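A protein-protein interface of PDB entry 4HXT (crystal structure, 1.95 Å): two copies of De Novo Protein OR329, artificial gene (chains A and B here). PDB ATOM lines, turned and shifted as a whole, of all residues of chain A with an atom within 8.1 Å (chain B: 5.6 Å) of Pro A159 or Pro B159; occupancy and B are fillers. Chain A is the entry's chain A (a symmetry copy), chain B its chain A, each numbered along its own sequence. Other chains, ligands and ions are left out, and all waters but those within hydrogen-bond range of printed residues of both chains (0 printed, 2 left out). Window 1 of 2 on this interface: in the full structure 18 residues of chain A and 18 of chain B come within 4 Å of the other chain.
Among the printed residues, 11 pairs touch across the chains. Among the printed residues, Asp or Glu carboxylates within 4 Å of a Lys or Arg side-chain nitrogen of the other chain: Lys A122 with Glu B161 (3.6 Å).
OD2 of Asp A118 touches N of Pro B159 (3.8 Å). Asp B160 touches Lys A122. Asp B118 touches Pro A159. Pro A159 touches Pro B159. Gly A200 touches Glu B119. CD of Pro A201 touches OE2 of Glu B119, at 3.6 Å.
Asp B118 touches its own counterpart, Asp A118. Asp A118 touches Pro B159, and with the chains exchanged Pro A159 touches Asp B118. Pro B159 touches its own counterpart, Pro A159. Glu A161 touches its own counterpart, Glu B161. Positions printed for both chains: 118, 119, 121, 155, 157, 158, 159, 160, 161, 162, 163 and 164.
Pro A159 touches just these residues of chain B: Asp B118 and Pro B159. Of chain A, only Asp A118 (3.8 Å) and Pro A159 (3.4 Å) come within 4 Å of Pro B159. No residue of chain A comes within 4 Å of Gly B158. Printed residues of chain B within 4 Å of Gly A200: Glu B119 (3.8 Å). Of the printed residues of chain A, Asp B118 touches Asp A118 and Pro A159. Of the printed residues of chain A, Asp B160 touches Glu A119 (2.6 Å) and Lys A122 (3.4 Å). Of the printed residues of chain B, Asp A118 touches Asp B118 (2.4 Å) and Pro B159 (3.8 Å). Ile A166 touches none of the printed residues of chain B. The nearest printed residue of chain A that does not touch Asp B118 is Gly A158 (4.03 Å).
The side-chain carboxylate (OD2) of Asp B118 sits close to the side-chain carboxylate (OD2) of Asp A118, at 2.4 Å. OD1 of Asp A160 sits close to OE2 of Glu B119. OE2 of Glu A119 sits close to OD1 of Asp B160. NZ of Lys A122 lies within salt-bridge range of OE2 of Glu B161 (3.6 Å). OE1 of Glu B161 lies close to OE1 of Glu A161 (2.9 Å).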
ATOM      1  N   GLY A 116     -16.648  -7.719 -18.907  1.00  0.00           N
ATOM      2  CA  GLY A 116     -15.750  -7.048 -19.830  1.00  0.00           C
ATOM      3  C   GLY A 116     -14.556  -7.877 -20.270  1.00  0.00           C
ATOM      4  O   GLY A 116     -14.579  -9.104 -20.172  1.00  0.00           O
ATOM      5  N   PRO A 117     -13.495  -7.228 -20.776  1.00  0.00           N
ATOM      6  CA  PRO A 117     -12.269  -7.884 -21.244  1.00  0.00           C
ATOM      7  C   PRO A 117     -11.600  -8.704 -20.141  1.00  0.00           C
ATOM      8  O   PRO A 117     -11.898  -8.523 -18.959  1.00  0.00           O
ATOM      9  CB  PRO A 117     -11.394  -6.709 -21.675  1.00  0.00           C
ATOM     10  CG  PRO A 117     -12.387  -5.683 -22.088  1.00  0.00           C
ATOM     11  CD  PRO A 117     -13.419  -5.775 -21.000  1.00  0.00           C
ATOM     12  N   ASP A 118     -10.696  -9.598 -20.531  1.00  0.00           N
ATOM     13  CA  ASP A 118      -9.986 -10.428 -19.567  1.00  0.00           C
ATOM     14  C   ASP A 118      -9.209  -9.593 -18.549  1.00  0.00           C
ATOM     15  O   ASP A 118      -9.062  -9.998 -17.402  1.00  0.00           O
ATOM     16  CB  ASP A 118      -9.014 -11.383 -20.273  1.00  0.00           C
ATOM     17  CG  ASP A 118      -9.703 -12.605 -20.855  1.00  0.00           C
ATOM     18  OD1 ASP A 118     -10.848 -12.891 -20.448  1.00  0.00           O
ATOM     19  OD2 ASP A 118      -9.091 -13.290 -21.707  1.00  0.00           O
ATOM     20  N   GLU A 119      -8.697  -8.439 -18.973  1.00  0.00           N
ATOM     21  CA  GLU A 119      -7.948  -7.576 -18.064  1.00  0.00           C
ATOM     22  C   GLU A 119      -8.848  -7.053 -16.950  1.00  0.00           C
ATOM     23  O   GLU A 119      -8.388  -6.838 -15.827  1.00  0.00           O
ATOM     24  CB  GLU A 119      -7.333  -6.391 -18.815  1.00  0.00           C
ATOM     25  CG  GLU A 119      -6.197  -6.753 -19.772  1.00  0.00           C
ATOM     26  CD  GLU A 119      -4.940  -7.220 -19.045  1.00  0.00           C
ATOM     27  OE1 GLU A 119      -4.759  -6.856 -17.865  1.00  0.00           O
ATOM     28  OE2 GLU A 119      -4.125  -7.939 -19.659  1.00  0.00           O
ATOM     29  N   ALA A 120     -10.129  -6.856 -17.250  1.00  0.00           N
ATOM     30  CA  ALA A 120     -11.068  -6.360 -16.243  1.00  0.00           C
ATOM     31  C   ALA A 120     -11.323  -7.443 -15.198  1.00  0.00           C
ATOM     32  O   ALA A 120     -11.397  -7.165 -13.999  1.00  0.00           O
ATOM     33  CB  ALA A 120     -12.380  -5.936 -16.902  1.00  0.00           C
ATOM     34  N   ILE A 121     -11.448  -8.684 -15.656  1.00  0.00           N
ATOM     35  CA  ILE A 121     -11.684  -9.803 -14.751  1.00  0.00           C
ATOM     36  C   ILE A 121     -10.448 -10.016 -13.870  1.00  0.00           C
ATOM     37  O   ILE A 121     -10.564 -10.276 -12.672  1.00  0.00           O
ATOM     38  CB  ILE A 121     -11.995 -11.088 -15.543  1.00  0.00           C
ATOM     39  CG1 ILE A 121     -13.312 -10.907 -16.311  1.00  0.00           C
ATOM     40  CG2 ILE A 121     -12.072 -12.281 -14.607  1.00  0.00           C
ATOM     41  CD1 ILE A 121     -13.672 -12.072 -17.201  1.00  0.00           C
ATOM     42  N   LYS A 122      -9.267  -9.890 -14.469  1.00  0.00           N
ATOM     43  CA  LYS A 122      -8.022 -10.055 -13.727  1.00  0.00           C
ATOM     44  C   LYS A 122      -7.942  -9.047 -12.585  1.00  0.00           C
ATOM     45  O   LYS A 122      -7.466  -9.368 -11.497  1.00  0.00           O
ATOM     46  CB  LYS A 122      -6.816  -9.875 -14.657  1.00  0.00           C
ATOM     47  CG  LYS A 122      -5.472  -9.942 -13.937  1.00  0.00           C
ATOM     48  CD  LYS A 122      -4.314  -9.880 -14.919  1.00  0.00           C
ATOM     49  CE  LYS A 122      -2.978  -9.747 -14.196  1.00  0.00           C
ATOM     50  NZ  LYS A 122      -2.736 -10.880 -13.272  1.00  0.00           N
ATOM     51  N   VAL A 125      -9.871 -10.395  -9.730  1.00  0.00           N
ATOM     52  CA  VAL A 125      -9.179 -11.519  -9.107  1.00  0.00           C
ATOM     53  C   VAL A 125      -8.020 -11.029  -8.243  1.00  0.00           C
ATOM     54  O   VAL A 125      -7.872 -11.445  -7.094  1.00  0.00           O
ATOM     55  CB  VAL A 125      -8.616 -12.497 -10.168  1.00  0.00           C
ATOM     56  CG1 VAL A 125      -7.807 -13.593  -9.485  1.00  0.00           C
ATOM     57  CG2 VAL A 125      -9.757 -13.113 -10.975  1.00  0.00           C
ATOM     58  N   ASN A 154     -19.674 -14.629 -14.600  1.00  0.00           N
ATOM     59  CA  ASN A 154     -18.959 -13.815 -15.580  1.00  0.00           C
ATOM     60  C   ASN A 154     -17.459 -13.966 -15.414  1.00  0.00           C
ATOM     61  O   ASN A 154     -16.718 -14.064 -16.394  1.00  0.00           O
ATOM     62  CB  ASN A 154     -19.361 -12.345 -15.450  1.00  0.00           C
ATOM     63  CG  ASN A 154     -20.797 -12.104 -15.863  1.00  0.00           C
ATOM     64  OD1 ASN A 154     -21.448 -13.000 -16.399  1.00  0.00           O
ATOM     65  ND2 ASN A 154     -21.298 -10.895 -15.625  1.00  0.00           N
ATOM     66  N   ILE A 155     -17.007 -13.982 -14.166  1.00  0.00           N
ATOM     67  CA  ILE A 155     -15.588 -14.148 -13.893  1.00  0.00           C
ATOM     68  C   ILE A 155     -15.118 -15.486 -14.463  1.00  0.00           C
ATOM     69  O   ILE A 155     -14.035 -15.578 -15.037  1.00  0.00           O
ATOM     70  CB  ILE A 155     -15.322 -14.100 -12.372  1.00  0.00           C
ATOM     71  CG1 ILE A 155     -15.509 -12.666 -11.870  1.00  0.00           C
ATOM     72  CG2 ILE A 155     -13.931 -14.626 -12.055  1.00  0.00           C
ATOM     73  CD1 ILE A 155     -15.440 -12.522 -10.367  1.00  0.00           C
ATOM     74  N   ALA A 156     -15.951 -16.514 -14.322  1.00  0.00           N
ATOM     75  CA  ALA A 156     -15.620 -17.855 -14.807  1.00  0.00           C
ATOM     76  C   ALA A 156     -15.544 -17.966 -16.330  1.00  0.00           C
ATOM     77  O   ALA A 156     -15.135 -18.998 -16.857  1.00  0.00           O
ATOM     78  CB  ALA A 156     -16.624 -18.870 -14.263  1.00  0.00           C
ATOM     79  N   SER A 157     -15.940 -16.913 -17.041  1.00  0.00           N
ATOM     80  CA  SER A 157     -15.874 -16.935 -18.495  1.00  0.00           C
ATOM     81  C   SER A 157     -14.538 -16.353 -18.954  1.00  0.00           C
ATOM     82  O   SER A 157     -14.281 -16.249 -20.149  1.00  0.00           O
ATOM     83  CB  SER A 157     -17.016 -16.111 -19.097  1.00  0.00           C
ATOM     84  OG  SER A 157     -16.797 -14.728 -18.892  1.00  0.00           O
ATOM     85  N   GLY A 158     -13.690 -15.984 -18.000  1.00  0.00           N
ATOM     86  CA  GLY A 158     -12.407 -15.397 -18.342  1.00  0.00           C
ATOM     87  C   GLY A 158     -11.254 -16.373 -18.481  1.00  0.00           C
ATOM     88  O   GLY A 158     -11.454 -17.542 -18.797  1.00  0.00           O
ATOM     89  N   PRO A 159     -10.018 -15.912 -18.242  1.00  0.00           N
ATOM     90  CA  PRO A 159      -8.836 -16.769 -18.350  1.00  0.00           C
ATOM     91  C   PRO A 159      -8.765 -17.876 -17.304  1.00  0.00           C
ATOM     92  O   PRO A 159      -9.538 -17.897 -16.344  1.00  0.00           O
ATOM     93  CB  PRO A 159      -7.680 -15.777 -18.231  1.00  0.00           C
ATOM     94  CG  PRO A 159      -8.238 -14.725 -17.340  1.00  0.00           C
ATOM     95  CD  PRO A 159      -9.641 -14.538 -17.865  1.00  0.00           C
ATOM     96  N   ASP A 160      -7.824 -18.792 -17.505  1.00  0.00           N
ATOM     97  CA  ASP A 160      -7.612 -19.916 -16.598  1.00  0.00           C
ATOM     98  C   ASP A 160      -7.448 -19.463 -15.151  1.00  0.00           C
ATOM     99  O   ASP A 160      -8.041 -20.038 -14.239  1.00  0.00           O
ATOM    100  CB  ASP A 160      -6.361 -20.692 -17.020  1.00  0.00           C
ATOM    101  CG  ASP A 160      -6.162 -21.962 -16.215  1.00  0.00           C
ATOM    102  OD1 ASP A 160      -6.836 -22.968 -16.517  1.00  0.00           O
ATOM    103  OD2 ASP A 160      -5.340 -21.951 -15.275  1.00  0.00           O
ATOM    104  N   GLU A 161      -6.638 -18.429 -14.950  1.00  0.00           N
ATOM    105  CA  GLU A 161      -6.361 -17.893 -13.616  1.00  0.00           C
ATOM    106  C   GLU A 161      -7.624 -17.518 -12.838  1.00  0.00           C
ATOM    107  O   GLU A 161      -7.690 -17.706 -11.624  1.00  0.00           O
ATOM    108  CB  GLU A 161      -5.464 -16.653 -13.718  1.00  0.00           C
ATOM    109  CG  GLU A 161      -4.054 -16.899 -14.254  1.00  0.00           C
ATOM    110  CD  GLU A 161      -4.033 -17.366 -15.698  1.00  0.00           C
ATOM    111  OE1 GLU A 161      -4.784 -16.798 -16.522  1.00  0.00           O
ATOM    112  OE2 GLU A 161      -3.252 -18.291 -16.015  1.00  0.00           O
ATOM    113  N   ALA A 162      -8.613 -16.976 -13.542  1.00  0.00           N
ATOM    114  CA  ALA A 162      -9.869 -16.563 -12.929  1.00  0.00           C
ATOM    115  C   ALA A 162     -10.653 -17.773 -12.410  1.00  0.00           C
ATOM    116  O   ALA A 162     -11.194 -17.745 -11.306  1.00  0.00           O
ATOM    117  CB  ALA A 162     -10.717 -15.772 -13.949  1.00  0.00           C
ATOM    118  N   ILE A 163     -10.726 -18.830 -13.213  1.00  0.00           N
ATOM    119  CA  ILE A 163     -11.443 -20.035 -12.805  1.00  0.00           C
ATOM    120  C   ILE A 163     -10.707 -20.703 -11.638  1.00  0.00           C
ATOM    121  O   ILE A 163     -11.321 -21.182 -10.688  1.00  0.00           O
ATOM    122  CB  ILE A 163     -11.576 -21.027 -13.994  1.00  0.00           C
ATOM    123  CG1 ILE A 163     -12.506 -20.427 -15.056  1.00  0.00           C
ATOM    124  CG2 ILE A 163     -12.073 -22.374 -13.505  1.00  0.00           C
ATOM    125  CD1 ILE A 163     -12.669 -21.273 -16.308  1.00  0.00           C
ATOM    126  N   LYS A 164      -9.384 -20.726 -11.715  1.00  0.00           N
ATOM    127  CA  LYS A 164      -8.574 -21.312 -10.659  1.00  0.00           C
ATOM    128  C   LYS A 164      -8.852 -20.583  -9.349  1.00  0.00           C
ATOM    129  O   LYS A 164      -8.906 -21.203  -8.294  1.00  0.00           O
ATOM    130  CB  LYS A 164      -7.097 -21.200 -11.012  1.00  0.00           C
ATOM    131  CG  LYS A 164      -6.144 -21.758  -9.964  1.00  0.00           C
ATOM    132  CD  LYS A 164      -4.702 -21.538 -10.398  1.00  0.00           C
ATOM    133  CE  LYS A 164      -3.698 -22.346  -9.579  1.00  0.00           C
ATOM    134  NZ  LYS A 164      -3.448 -21.794  -8.217  1.00  0.00           N
ATOM    135  N   ALA A 165      -9.040 -19.269  -9.427  1.00  0.00           N
ATOM    136  CA  ALA A 165      -9.322 -18.458  -8.245  1.00  0.00           C
ATOM    137  C   ALA A 165     -10.649 -18.878  -7.607  1.00  0.00           C
ATOM    138  O   ALA A 165     -10.768 -18.942  -6.379  1.00  0.00           O
ATOM    139  CB  ALA A 165      -9.348 -16.971  -8.621  1.00  0.00           C
ATOM    140  N   ILE A 166     -11.641 -19.175  -8.442  1.00  0.00           N
ATOM    141  CA  ILE A 166     -12.941 -19.599  -7.943  1.00  0.00           C
ATOM    142  C   ILE A 166     -12.800 -20.952  -7.262  1.00  0.00           C
ATOM    143  O   ILE A 166     -13.368 -21.189  -6.201  1.00  0.00           O
ATOM    144  CB  ILE A 166     -13.975 -19.726  -9.088  1.00  0.00           C
ATOM    145  CG1 ILE A 166     -14.214 -18.357  -9.731  1.00  0.00           C
ATOM    146  CG2 ILE A 166     -15.284 -20.304  -8.544  1.00  0.00           C
ATOM    147  CD1 ILE A 166     -15.161 -18.382 -10.925  1.00  0.00           C
ATOM    148  N   ASN A 196     -19.480 -22.543 -17.083  1.00  0.00           N
ATOM    149  CA  ASN A 196     -18.308 -21.762 -17.462  1.00  0.00           C
ATOM    150  C   ASN A 196     -17.051 -22.300 -16.796  1.00  0.00           C
ATOM    151  O   ASN A 196     -16.000 -22.408 -17.426  1.00  0.00           O
ATOM    152  CB  ASN A 196     -18.520 -20.288 -17.110  1.00  0.00           C
ATOM    153  CG  ASN A 196     -19.506 -19.614 -18.041  1.00  0.00           C
ATOM    154  OD1 ASN A 196     -19.843 -20.158 -19.092  1.00  0.00           O
ATOM    155  ND2 ASN A 196     -19.967 -18.429 -17.672  1.00  0.00           N
ATOM    156  N   GLY A 200     -13.019 -24.703 -18.218  1.00  0.00           N
ATOM    157  CA  GLY A 200     -11.671 -24.349 -17.819  1.00  0.00           C
ATOM    158  C   GLY A 200     -10.714 -25.525 -17.737  1.00  0.00           C
ATOM    159  O   GLY A 200     -10.854 -26.506 -18.471  1.00  0.00           O
ATOM    160  N   PRO A 201      -9.729 -25.457 -16.829  1.00  0.00           N
ATOM    161  CA  PRO A 201      -8.740 -26.522 -16.659  1.00  0.00           C
ATOM    162  C   PRO A 201      -9.340 -27.790 -16.077  1.00  0.00           C
ATOM    163  O   PRO A 201     -10.369 -27.754 -15.407  1.00  0.00           O
ATOM    164  CB  PRO A 201      -7.720 -25.886 -15.725  1.00  0.00           C
ATOM    165  CG  PRO A 201      -8.594 -25.067 -14.821  1.00  0.00           C
ATOM    166  CD  PRO A 201      -9.554 -24.411 -15.802  1.00  0.00           C
ATOM    167  N   ASP B 118      -9.139 -19.054 -24.449  1.00  0.00           N
ATOM    168  CA  ASP B 118      -7.986 -18.644 -23.658  1.00  0.00           C
ATOM    169  C   ASP B 118      -7.167 -19.839 -23.172  1.00  0.00           C
ATOM    170  O   ASP B 118      -5.952 -19.741 -23.038  1.00  0.00           O
ATOM    171  CB  ASP B 118      -8.419 -17.811 -22.444  1.00  0.00           C
ATOM    172  CG  ASP B 118      -8.722 -16.364 -22.797  1.00  0.00           C
ATOM    173  OD1 ASP B 118      -8.296 -15.916 -23.881  1.00  0.00           O
ATOM    174  OD2 ASP B 118      -9.372 -15.671 -21.980  1.00  0.00           O
ATOM    175  N   GLU B 119      -7.831 -20.959 -22.892  1.00  0.00           N
ATOM    176  CA  GLU B 119      -7.124 -22.149 -22.430  1.00  0.00           C
ATOM    177  C   GLU B 119      -6.191 -22.680 -23.514  1.00  0.00           C
ATOM    178  O   GLU B 119      -5.135 -23.237 -23.209  1.00  0.00           O
ATOM    179  CB  GLU B 119      -8.110 -23.252 -22.029  1.00  0.00           C
ATOM    180  CG  GLU B 119      -8.919 -22.963 -20.764  1.00  0.00           C
ATOM    181  CD  GLU B 119      -8.063 -22.973 -19.501  1.00  0.00           C
ATOM    182  OE1 GLU B 119      -6.996 -23.618 -19.505  1.00  0.00           O
ATOM    183  OE2 GLU B 119      -8.466 -22.347 -18.499  1.00  0.00           O
ATOM    184  N   ILE B 121      -4.638 -20.813 -25.794  1.00  0.00           N
ATOM    185  CA  ILE B 121      -3.506 -19.897 -25.854  1.00  0.00           C
ATOM    186  C   ILE B 121      -2.560 -20.176 -24.681  1.00  0.00           C
ATOM    187  O   ILE B 121      -1.339 -20.164 -24.837  1.00  0.00           O
ATOM    188  CB  ILE B 121      -3.986 -18.433 -25.807  1.00  0.00           C
ATOM    189  CG1 ILE B 121      -4.817 -18.130 -27.062  1.00  0.00           C
ATOM    190  CG2 ILE B 121      -2.801 -17.490 -25.700  1.00  0.00           C
ATOM    191  CD1 ILE B 121      -5.422 -16.746 -27.081  1.00  0.00           C
ATOM    192  N   ILE B 155      -2.136 -14.826 -30.161  1.00  0.00           N
ATOM    193  CA  ILE B 155      -1.786 -15.059 -28.769  1.00  0.00           C
ATOM    194  C   ILE B 155      -2.013 -13.775 -27.970  1.00  0.00           C
ATOM    195  O   ILE B 155      -2.514 -13.815 -26.849  1.00  0.00           O
ATOM    196  CB  ILE B 155      -0.309 -15.499 -28.649  1.00  0.00           C
ATOM    197  CG1 ILE B 155      -0.161 -16.925 -29.188  1.00  0.00           C
ATOM    198  CG2 ILE B 155       0.166 -15.394 -27.208  1.00  0.00           C
ATOM    199  CD1 ILE B 155       1.268 -17.407 -29.279  1.00  0.00           C
ATOM    200  N   SER B 157      -4.212 -11.667 -28.238  1.00  0.00           N
ATOM    201  CA  SER B 157      -5.619 -11.342 -28.046  1.00  0.00           C
ATOM    202  C   SER B 157      -6.158 -12.104 -26.836  1.00  0.00           C
ATOM    203  O   SER B 157      -7.335 -12.001 -26.507  1.00  0.00           O
ATOM    204  CB  SER B 157      -6.433 -11.726 -29.285  1.00  0.00           C
ATOM    205  OG  SER B 157      -6.548 -13.132 -29.393  1.00  0.00           O
ATOM    206  N   GLY B 158      -5.289 -12.861 -26.174  1.00  0.00           N
ATOM    207  CA  GLY B 158      -5.717 -13.640 -25.026  1.00  0.00           C
ATOM    208  C   GLY B 158      -5.587 -12.954 -23.679  1.00  0.00           C
ATOM    209  O   GLY B 158      -5.629 -11.730 -23.591  1.00  0.00           O
ATOM    210  N   PRO B 159      -5.422 -13.731 -22.599  1.00  0.00           N
ATOM    211  CA  PRO B 159      -5.290 -13.170 -21.253  1.00  0.00           C
ATOM    212  C   PRO B 159      -4.013 -12.367 -21.030  1.00  0.00           C
ATOM    213  O   PRO B 159      -3.100 -12.378 -21.858  1.00  0.00           O
ATOM    214  CB  PRO B 159      -5.368 -14.405 -20.357  1.00  0.00           C
ATOM    215  CG  PRO B 159      -4.765 -15.467 -21.206  1.00  0.00           C
ATOM    216  CD  PRO B 159      -5.364 -15.203 -22.566  1.00  0.00           C
ATOM    217  N   ASP B 160      -3.965 -11.675 -19.898  1.00  0.00           N
ATOM    218  CA  ASP B 160      -2.815 -10.857 -19.522  1.00  0.00           C
ATOM    219  C   ASP B 160      -1.509 -11.642 -19.585  1.00  0.00           C
ATOM    220  O   ASP B 160      -0.507 -11.159 -20.112  1.00  0.00           O
ATOM    221  CB  ASP B 160      -3.005 -10.321 -18.100  1.00  0.00           C
ATOM    222  CG  ASP B 160      -1.920  -9.341 -17.697  1.00  0.00           C
ATOM    223  OD1 ASP B 160      -2.001  -8.165 -18.106  1.00  0.00           O
ATOM    224  OD2 ASP B 160      -0.983  -9.749 -16.980  1.00  0.00           O
ATOM    225  N   GLU B 161      -1.528 -12.854 -19.040  1.00  0.00           N
ATOM    226  CA  GLU B 161      -0.347 -13.720 -19.003  1.00  0.00           C
ATOM    227  C   GLU B 161       0.281 -13.951 -20.377  1.00  0.00           C
ATOM    228  O   GLU B 161       1.502 -14.024 -20.503  1.00  0.00           O
ATOM    229  CB  GLU B 161      -0.706 -15.081 -18.393  1.00  0.00           C
ATOM    230  CG  GLU B 161      -1.124 -15.058 -16.924  1.00  0.00           C
ATOM    231  CD  GLU B 161      -2.419 -14.304 -16.678  1.00  0.00           C
ATOM    232  OE1 GLU B 161      -3.376 -14.487 -17.463  1.00  0.00           O
ATOM    233  OE2 GLU B 161      -2.486 -13.540 -15.690  1.00  0.00           O
ATOM    234  N   ALA B 162      -0.562 -14.080 -21.398  1.00  0.00           N
ATOM    235  CA  ALA B 162      -0.102 -14.313 -22.761  1.00  0.00           C
ATOM    236  C   ALA B 162       0.658 -13.098 -23.303  1.00  0.00           C
ATOM    237  O   ALA B 162       1.708 -13.241 -23.928  1.00  0.00           O
ATOM    238  CB  ALA B 162      -1.305 -14.642 -23.673  1.00  0.00           C
ATOM    239  N   ILE B 163       0.122 -11.903 -23.073  1.00  0.00           N
ATOM    240  CA  ILE B 163       0.776 -10.685 -23.541  1.00  0.00           C
ATOM    241  C   ILE B 163       2.090 -10.479 -22.778  1.00  0.00           C
ATOM    242  O   ILE B 163       3.105 -10.091 -23.350  1.00  0.00           O
ATOM    243  CB  ILE B 163      -0.153  -9.453 -23.352  1.00  0.00           C
ATOM    244  CG1 ILE B 163      -1.355  -9.572 -24.298  1.00  0.00           C
ATOM    245  CG2 ILE B 163       0.620  -8.168 -23.581  1.00  0.00           C
ATOM    246  CD1 ILE B 163      -2.380  -8.458 -24.165  1.00  0.00           C
ATOM    247  N   LYS B 164       2.063 -10.749 -21.480  1.00  0.00           N
ATOM    248  CA  LYS B 164       3.252 -10.613 -20.654  1.00  0.00           C
ATOM    249  C   LYS B 164       4.346 -11.527 -21.196  1.00  0.00           C
ATOM    250  O   LYS B 164       5.515 -11.158 -21.201  1.00  0.00           O
ATOM    251  CB  LYS B 164       2.930 -10.985 -19.213  1.00  0.00           C
ATOM    252  CG  LYS B 164       4.109 -10.908 -18.253  1.00  0.00           C
ATOM    253  CD  LYS B 164       3.682 -11.358 -16.863  1.00  0.00           C
ATOM    254  CE  LYS B 164       4.699 -11.006 -15.780  1.00  0.00           C
ATOM    255  NZ  LYS B 164       5.902 -11.885 -15.773  1.00  0.00           N
